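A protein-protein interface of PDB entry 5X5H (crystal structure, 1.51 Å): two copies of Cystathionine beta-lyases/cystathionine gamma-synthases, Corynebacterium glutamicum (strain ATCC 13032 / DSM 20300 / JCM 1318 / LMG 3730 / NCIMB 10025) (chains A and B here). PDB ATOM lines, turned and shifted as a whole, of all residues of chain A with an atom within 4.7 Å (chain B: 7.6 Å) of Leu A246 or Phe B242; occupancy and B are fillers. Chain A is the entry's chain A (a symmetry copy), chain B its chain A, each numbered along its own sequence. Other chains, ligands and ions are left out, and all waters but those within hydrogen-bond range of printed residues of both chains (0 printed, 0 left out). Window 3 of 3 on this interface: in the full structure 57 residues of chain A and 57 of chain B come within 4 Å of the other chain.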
ATOM      1  N   VAL A 212      19.096  29.364  -3.680  1.00  0.00           N
ATOM      2  CA  VAL A 212      18.944  27.946  -3.300  1.00  0.00           C
ATOM      3  C   VAL A 212      20.183  27.177  -3.816  1.00  0.00           C
ATOM      4  O   VAL A 212      20.444  27.176  -5.014  1.00  0.00           O
ATOM      5  CB  VAL A 212      17.623  27.306  -3.760  1.00  0.00           C
ATOM      6  CG1 VAL A 212      17.209  27.693  -5.147  1.00  0.00           C
ATOM      7  CG2 VAL A 212      17.650  25.828  -3.620  1.00  0.00           C
ATOM      8  N   PHE A 242      11.373  23.009   0.474  1.00  0.00           N
ATOM      9  CA  PHE A 242      11.249  24.431   0.148  1.00  0.00           C
ATOM     10  C   PHE A 242      12.241  24.719  -0.960  1.00  0.00           C
ATOM     11  O   PHE A 242      11.932  25.459  -1.906  1.00  0.00           O
ATOM     12  CB  PHE A 242      11.554  25.321   1.409  1.00  0.00           C
ATOM     13  CG  PHE A 242      10.566  25.192   2.463  1.00  0.00           C
ATOM     14  CD1 PHE A 242       9.388  25.964   2.429  1.00  0.00           C
ATOM     15  CD2 PHE A 242      10.731  24.248   3.483  1.00  0.00           C
ATOM     16  CE1 PHE A 242       8.369  25.797   3.381  1.00  0.00           C
ATOM     17  CE2 PHE A 242       9.704  24.122   4.440  1.00  0.00           C
ATOM     18  CZ  PHE A 242       8.594  24.880   4.368  1.00  0.00           C
ATOM     19  N   ASP A 243      13.462  24.217  -0.858  1.00  0.00           N
ATOM     20  CA  ASP A 243      14.479  24.486  -1.891  1.00  0.00           C
ATOM     21  C   ASP A 243      14.052  23.841  -3.190  1.00  0.00           C
ATOM     22  O   ASP A 243      14.222  24.429  -4.263  1.00  0.00           O
ATOM     23  CB  ASP A 243      15.813  23.953  -1.444  1.00  0.00           C
ATOM     24  CG  ASP A 243      16.482  24.903  -0.411  1.00  0.00           C
ATOM     25  OD1 ASP A 243      15.904  25.954  -0.013  1.00  0.00           O
ATOM     26  OD2 ASP A 243      17.623  24.554  -0.066  1.00  0.00           O
ATOM     27  N   ALA A 244      13.526  22.608  -3.196  1.00  0.00           N
ATOM     28  CA  ALA A 244      13.122  21.962  -4.458  1.00  0.00           C
ATOM     29  C   ALA A 244      11.974  22.747  -5.092  1.00  0.00           C
ATOM     30  O   ALA A 244      11.932  22.873  -6.342  1.00  0.00           O
ATOM     31  CB  ALA A 244      12.638  20.574  -4.209  1.00  0.00           C
ATOM     32  N   TYR A 245      11.067  23.326  -4.322  1.00  0.00           N
ATOM     33  CA  TYR A 245      10.027  24.191  -4.876  1.00  0.00           C
ATOM     34  C   TYR A 245      10.630  25.447  -5.494  1.00  0.00           C
ATOM     35  O   TYR A 245      10.278  25.802  -6.653  1.00  0.00           O
ATOM     36  CB  TYR A 245       9.019  24.632  -3.757  1.00  0.00           C
ATOM     37  CG  TYR A 245       7.977  25.564  -4.342  1.00  0.00           C
ATOM     38  CD1 TYR A 245       6.940  25.084  -5.051  1.00  0.00           C
ATOM     39  CD2 TYR A 245       8.122  26.925  -4.192  1.00  0.00           C
ATOM     40  CE1 TYR A 245       6.031  25.871  -5.663  1.00  0.00           C
ATOM     41  CE2 TYR A 245       7.235  27.792  -4.831  1.00  0.00           C
ATOM     42  CZ  TYR A 245       6.197  27.232  -5.600  1.00  0.00           C
ATOM     43  OH  TYR A 245       5.283  28.075  -6.314  1.00  0.00           O
ATOM     44  N   LEU A 246      11.544  26.103  -4.791  1.00  0.00           N
ATOM     45  CA  LEU A 246      12.191  27.337  -5.295  1.00  0.00           C
ATOM     46  C   LEU A 246      13.013  27.099  -6.555  1.00  0.00           C
ATOM     47  O   LEU A 246      13.036  27.922  -7.486  1.00  0.00           O
ATOM     48  CB  LEU A 246      13.005  28.046  -4.236  1.00  0.00           C
ATOM     49  CG  LEU A 246      12.126  28.684  -3.167  1.00  0.00           C
ATOM     50  CD1 LEU A 246      13.146  29.070  -2.103  1.00  0.00           C
ATOM     51  CD2 LEU A 246      11.335  29.857  -3.707  1.00  0.00           C
ATOM     52  N   THR A 247      13.751  25.997  -6.564  1.00  0.00           N
ATOM     53  CA  THR A 247      14.514  25.599  -7.738  1.00  0.00           C
ATOM     54  C   THR A 247      13.573  25.435  -8.932  1.00  0.00           C
ATOM     55  O   THR A 247      13.859  25.931 -10.058  1.00  0.00           O
ATOM     56  CB  THR A 247      15.379  24.364  -7.519  1.00  0.00           C
ATOM     57  OG1 THR A 247      16.275  24.559  -6.383  1.00  0.00           O
ATOM     58  CG2 THR A 247      16.177  23.976  -8.778  1.00  0.00           C
ATOM     59  N   ALA A 248      12.536  24.615  -8.774  1.00  0.00           N
ATOM     60  CA  ALA A 248      11.578  24.429  -9.873  1.00  0.00           C
ATOM     61  C   ALA A 248      10.900  25.697 -10.261  1.00  0.00           C
ATOM     62  O   ALA A 248      10.628  25.900 -11.444  1.00  0.00           O
ATOM     63  CB  ALA A 248      10.576  23.385  -9.452  1.00  0.00           C
ATOM     64  N   ARG A 249      10.618  26.588  -9.316  1.00  0.00           N
ATOM     65  CA  ARG A 249      10.042  27.885  -9.653  1.00  0.00           C
ATOM     66  C   ARG A 249      10.949  28.706 -10.584  1.00  0.00           C
ATOM     67  O   ARG A 249      10.538  29.240 -11.563  1.00  0.00           O
ATOM     68  CB  ARG A 249       9.728  28.654  -8.350  1.00  0.00           C
ATOM     69  CG  ARG A 249       9.005  30.017  -8.598  1.00  0.00           C
ATOM     70  CD  ARG A 249       8.931  30.777  -7.303  1.00  0.00           C
ATOM     71  NE  ARG A 249       7.925  31.786  -7.219  1.00  0.00           N
ATOM     72  CZ  ARG A 249       8.059  33.129  -7.294  1.00  0.00           C
ATOM     73  NH1 ARG A 249       9.224  33.661  -7.650  1.00  0.00           N
ATOM     74  NH2 ARG A 249       7.071  33.884  -6.957  1.00  0.00           N
ATOM     75  N   GLY A 250      12.233  28.730 -10.180  1.00  0.00           N
ATOM     76  CA  GLY A 250      13.183  29.391 -11.017  1.00  0.00           C
ATOM     77  C   GLY A 250      13.289  28.788 -12.388  1.00  0.00           C
ATOM     78  O   GLY A 250      13.471  29.496 -13.420  1.00  0.00           O
ATOM     79  N   ILE B  32      16.494  34.914   7.639  1.00  0.00           N
ATOM     80  CA  ILE B  32      16.640  33.807   6.721  1.00  0.00           C
ATOM     81  C   ILE B  32      17.488  34.303   5.566  1.00  0.00           C
ATOM     82  O   ILE B  32      16.952  35.116   4.731  1.00  0.00           O
ATOM     83  CB  ILE B  32      15.302  33.189   6.333  1.00  0.00           C
ATOM     84  CG1 ILE B  32      14.613  32.696   7.591  1.00  0.00           C
ATOM     85  CG2 ILE B  32      15.558  32.035   5.381  1.00  0.00           C
ATOM     86  CD1 ILE B  32      13.154  32.330   7.306  1.00  0.00           C
ATOM     87  N   TYR B  33      18.775  33.964   5.507  1.00  0.00           N
ATOM     88  CA  TYR B  33      19.624  34.479   4.451  1.00  0.00           C
ATOM     89  C   TYR B  33      19.599  33.564   3.236  1.00  0.00           C
ATOM     90  O   TYR B  33      20.497  32.795   2.962  1.00  0.00           O
ATOM     91  CB  TYR B  33      21.069  34.602   4.997  1.00  0.00           C
ATOM     92  CG  TYR B  33      21.256  35.746   5.978  1.00  0.00           C
ATOM     93  CD1 TYR B  33      21.445  37.012   5.483  1.00  0.00           C
ATOM     94  CD2 TYR B  33      21.127  35.627   7.344  1.00  0.00           C
ATOM     95  CE1 TYR B  33      21.589  38.063   6.324  1.00  0.00           C
ATOM     96  CE2 TYR B  33      21.260  36.699   8.210  1.00  0.00           C
ATOM     97  CZ  TYR B  33      21.473  37.912   7.675  1.00  0.00           C
ATOM     98  OH  TYR B  33      21.563  39.031   8.518  1.00  0.00           O
ATOM     99  N   ALA B  34      18.503  33.675   2.502  1.00  0.00           N
ATOM    100  CA  ALA B  34      18.323  32.934   1.251  1.00  0.00           C
ATOM    101  C   ALA B  34      19.030  33.521   0.061  1.00  0.00           C
ATOM    102  O   ALA B  34      18.468  34.213  -0.792  1.00  0.00           O
ATOM    103  CB  ALA B  34      16.801  32.716   0.965  1.00  0.00           C
ATOM    104  N   SER B  35      20.340  33.318   0.156  1.00  0.00           N
ATOM    105  CA  SER B  35      21.326  33.828  -0.759  1.00  0.00           C
ATOM    106  C   SER B  35      22.349  32.790  -0.912  1.00  0.00           C
ATOM    107  O   SER B  35      22.819  32.231   0.135  1.00  0.00           O
ATOM    108  CB  SER B  35      22.011  35.100  -0.302  1.00  0.00           C
ATOM    109  OG  SER B  35      21.173  36.234  -0.280  1.00  0.00           O
ATOM    110  N   THR B  59      22.402  31.811   8.890  1.00  0.00           N
ATOM    111  CA  THR B  59      21.174  31.175   9.371  1.00  0.00           C
ATOM    112  C   THR B  59      21.471  29.742   9.809  1.00  0.00           C
ATOM    113  O   THR B  59      20.993  29.299  10.842  1.00  0.00           O
ATOM    114  CB  THR B  59      20.085  31.183   8.328  1.00  0.00           C
ATOM    115  OG1 THR B  59      19.829  32.518   7.824  1.00  0.00           O
ATOM    116  CG2 THR B  59      18.806  30.528   8.840  1.00  0.00           C
ATOM    117  N   ILE B  60      22.343  29.077   9.085  1.00  0.00           N
ATOM    118  CA  ILE B  60      22.772  27.676   9.426  1.00  0.00           C
ATOM    119  C   ILE B  60      23.667  27.734  10.642  1.00  0.00           C
ATOM    120  O   ILE B  60      23.496  26.941  11.605  1.00  0.00           O
ATOM    121  CB  ILE B  60      23.478  27.030   8.218  1.00  0.00           C
ATOM    122  CG1 ILE B  60      22.537  27.022   7.025  1.00  0.00           C
ATOM    123  CG2 ILE B  60      24.002  25.643   8.596  1.00  0.00           C
ATOM    124  CD1 ILE B  60      23.158  26.499   5.717  1.00  0.00           C
ATOM    125  N   VAL B 212      10.935  18.952   8.733  1.00  0.00           N
ATOM    126  CA  VAL B 212      12.280  19.276   8.221  1.00  0.00           C
ATOM    127  C   VAL B 212      13.204  18.068   8.497  1.00  0.00           C
ATOM    128  O   VAL B 212      13.369  17.678   9.649  1.00  0.00           O
ATOM    129  CB  VAL B 212      12.862  20.594   8.762  1.00  0.00           C
ATOM    130  CG1 VAL B 212      12.611  20.816  10.222  1.00  0.00           C
ATOM    131  CG2 VAL B 212      14.309  20.721   8.460  1.00  0.00           C
ATOM    132  N   PRO B 239      22.302  21.797   4.853  1.00  0.00           N
ATOM    133  CA  PRO B 239      20.864  22.069   4.957  1.00  0.00           C
ATOM    134  C   PRO B 239      20.500  23.329   4.187  1.00  0.00           C
ATOM    135  O   PRO B 239      21.321  24.231   3.983  1.00  0.00           O
ATOM    136  CB  PRO B 239      20.657  22.310   6.447  1.00  0.00           C
ATOM    137  CG  PRO B 239      21.954  22.580   6.964  1.00  0.00           C
ATOM    138  CD  PRO B 239      23.019  22.199   6.033  1.00  0.00           C
ATOM    139  N   SER B 240      19.265  23.407   3.747  1.00  0.00           N
ATOM    140  CA  SER B 240      18.658  24.659   3.303  1.00  0.00           C
ATOM    141  C   SER B 240      18.595  25.683   4.424  1.00  0.00           C
ATOM    142  O   SER B 240      18.417  25.353   5.632  1.00  0.00           O
ATOM    143  CB  SER B 240      17.171  24.333   2.977  1.00  0.00           C
ATOM    144  OG  SER B 240      16.410  25.459   2.709  1.00  0.00           O
ATOM    145  N   VAL B 241      18.670  26.961   4.120  1.00  0.00           N
ATOM    146  CA  VAL B 241      18.513  28.000   5.117  1.00  0.00           C
ATOM    147  C   VAL B 241      17.101  27.979   5.671  1.00  0.00           C
ATOM    148  O   VAL B 241      16.858  28.289   6.837  1.00  0.00           O
ATOM    149  CB  VAL B 241      18.900  29.426   4.693  1.00  0.00           C
ATOM    150  CG1 VAL B 241      20.365  29.492   4.350  1.00  0.00           C
ATOM    151  CG2 VAL B 241      18.012  29.885   3.545  1.00  0.00           C
ATOM    152  N   PHE B 242      16.102  27.646   4.861  1.00  0.00           N
ATOM    153  CA  PHE B 242      14.724  27.600   5.352  1.00  0.00           C
ATOM    154  C   PHE B 242      14.652  26.469   6.359  1.00  0.00           C
ATOM    155  O   PHE B 242      14.007  26.602   7.411  1.00  0.00           O
ATOM    156  CB  PHE B 242      13.718  27.352   4.169  1.00  0.00           C
ATOM    157  CG  PHE B 242      13.639  28.456   3.232  1.00  0.00           C
ATOM    158  CD1 PHE B 242      12.784  29.546   3.491  1.00  0.00           C
ATOM    159  CD2 PHE B 242      14.465  28.494   2.103  1.00  0.00           C
ATOM    160  CE1 PHE B 242      12.753  30.674   2.656  1.00  0.00           C
ATOM    161  CE2 PHE B 242      14.393  29.627   1.268  1.00  0.00           C
ATOM    162  CZ  PHE B 242      13.561  30.646   1.555  1.00  0.00           C
ATOM    163  N   ASP B 243      15.236  25.320   6.058  1.00  0.00           N
ATOM    164  CA  ASP B 243      15.175  24.175   6.985  1.00  0.00           C
ATOM    165  C   ASP B 243      15.933  24.516   8.247  1.00  0.00           C
ATOM    166  O   ASP B 243      15.494  24.175   9.350  1.00  0.00           O
ATOM    167  CB  ASP B 243      15.757  22.954   6.327  1.00  0.00           C
ATOM    168  CG  ASP B 243      14.747  22.315   5.331  1.00  0.00           C
ATOM    169  OD1 ASP B 243      13.613  22.832   5.122  1.00  0.00           O
ATOM    170  OD2 ASP B 243      15.144  21.257   4.816  1.00  0.00           O
ATOM    171  N   ALA B 244      17.112  25.152   8.181  1.00  0.00           N
ATOM    172  CA  ALA B 244      17.869  25.475   9.405  1.00  0.00           C
ATOM    173  C   ALA B 244      17.075  26.468  10.253  1.00  0.00           C
ATOM    174  O   ALA B 244      17.096  26.361  11.506  1.00  0.00           O
ATOM    175  CB  ALA B 244      19.173  26.112   9.065  1.00  0.00           C
ATOM    176  N   TYR B 245      16.336  27.395   9.665  1.00  0.00           N
ATOM    177  CA  TYR B 245      15.462  28.282  10.430  1.00  0.00           C
ATOM    178  C   TYR B 245      14.342  27.499  11.105  1.00  0.00           C
ATOM    179  O   TYR B 245      14.101  27.688  12.329  1.00  0.00           O
ATOM    180  CB  TYR B 245      14.811  29.360   9.494  1.00  0.00           C
ATOM    181  CG  TYR B 245      13.874  30.239  10.298  1.00  0.00           C
ATOM    182  CD1 TYR B 245      14.350  31.234  11.069  1.00  0.00           C
ATOM    183  CD2 TYR B 245      12.521  29.985  10.282  1.00  0.00           C
ATOM    184  CE1 TYR B 245      13.571  31.992  11.867  1.00  0.00           C
ATOM    185  CE2 TYR B 245      11.668  30.711  11.113  1.00  0.00           C
ATOM    186  CZ  TYR B 245      12.230  31.707  11.934  1.00  0.00           C
ATOM    187  OH  TYR B 245      11.406  32.454  12.840  1.00  0.00           O
ATOM    188  N   LEU B 246      13.683  26.610  10.374  1.00  0.00           N
ATOM    189  CA  LEU B 246      12.574  25.798  10.929  1.00  0.00           C
ATOM    190  C   LEU B 246      13.027  24.870  12.048  1.00  0.00           C
ATOM    191  O   LEU B 246      12.325  24.668  13.054  1.00  0.00           O
ATOM    192  CB  LEU B 246      11.812  25.042   9.864  1.00  0.00           C
ATOM    193  CG  LEU B 246      10.982  25.969   8.984  1.00  0.00           C
ATOM    194  CD1 LEU B 246      10.556  25.039   7.855  1.00  0.00           C
ATOM    195  CD2 LEU B 246       9.822  26.582   9.739  1.00  0.00           C
ATOM    196  N   THR B 247      14.179  24.242  11.848  1.00  0.00           N
ATOM    197  CA  THR B 247      14.774  23.397  12.873  1.00  0.00           C
ATOM    198  C   THR B 247      15.003  24.213  14.145  1.00  0.00           C
ATOM    199  O   THR B 247      14.669  23.760  15.276  1.00  0.00           O
ATOM    200  CB  THR B 247      16.040  22.681  12.419  1.00  0.00           C
ATOM    201  OG1 THR B 247      15.784  21.901  11.211  1.00  0.00           O
ATOM    202  CG2 THR B 247      16.639  21.791  13.523  1.00  0.00           C
ATOM    203  N   ALA B 248      15.711  25.333  14.023  1.00  0.00           N
ATOM    204  CA  ALA B 248      15.949  26.179  15.202  1.00  0.00           C
ATOM    205  C   ALA B 248      14.686  26.688  15.804  1.00  0.00           C
ATOM    206  O   ALA B 248      14.604  26.809  17.027  1.00  0.00           O
ATOM    207  CB  ALA B 248      16.851  27.315  14.792  1.00  0.00           C
ATOM    208  N   ARG B 249      13.668  26.986  15.003  1.00  0.00           N
ATOM    209  CA  ARG B 249      12.378  27.397  15.546  1.00  0.00           C
ATOM    210  C   ARG B 249      11.751  26.321  16.446  1.00  0.00           C
ATOM    211  O   ARG B 249      11.306  26.571  17.520  1.00  0.00           O
ATOM    212  CB  ARG B 249      11.437  27.778  14.382  1.00  0.00           C
ATOM    213  CG  ARG B 249      10.059  28.338  14.862  1.00  0.00           C
ATOM    214  CD  ARG B 249       9.146  28.481  13.676  1.00  0.00           C
ATOM    215  NE  ARG B 249       8.056  29.391  13.823  1.00  0.00           N
ATOM    216  CZ  ARG B 249       6.747  29.124  14.028  1.00  0.00           C
ATOM    217  NH1 ARG B 249       6.358  27.882  14.298  1.00  0.00           N
ATOM    218  NH2 ARG B 249       5.880  30.067  13.896  1.00  0.00           N
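The side-chain carboxylate (OD1) of Asp A243 is in hydrogen-bond range of the side-chain hydroxyl (OG) of Ser B240, 2.8 Å away.
Val A212 touches none of the printed residues of chain B.
Of the printed residues of chain B, Asp A243 touches Ser B240 (2.8 Å) and Phe B242 (3.6 Å).
Printed residues of chain A within 4 Å of Ser B240: Asp A243.
Phe B242 touches two residues of chain A.
Printed residues of chain A within 4 Å of Asp B243: Phe A242.
Printed residues of chain A within 4 Å of Leu B246: Phe A242.
The nearest residue of chain A that does not touch Phe B242 is Phe A242 (4.1 Å).
Phe A242 touches Asp B243, and with the chains exchanged Asp A243 touches Phe B242.
Phe A242 touches Leu B246, and with the chains exchanged Leu A246 touches Phe B242.
9 positions are printed for both chains.
Asp B243 touches Phe A242.
Leu B246 touches Phe A242 (CD1 to CE2, 3.6 Å).
OD1 of Asp A243 touches CD2 of Phe B242, at 3.6 Å.
Phe B242 touches Leu A246 (CE2 to CD1, 3.6 Å).
The side-chain hydroxyl (OG) of Ser B240 is in hydrogen-bond range of the backbone NH (N) of Phe B242, 3.1 Å away.
The side-chain hydroxyl (OG1) of Thr B247 sits at hydrogen-bond distance from the backbone carbonyl oxygen (O) of Asp B243, 3.0 Å away.
The backbone carbonyl oxygen (O) of Asp A243 sits at hydrogen-bond distance from the side-chain hydroxyl (OG1) of Thr A247 (3.0 Å).
Of the 18 printed residues of chain B, 4 touch a printed residue of chain A.
Among the printed residues, 5 pairs touch across the chains.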
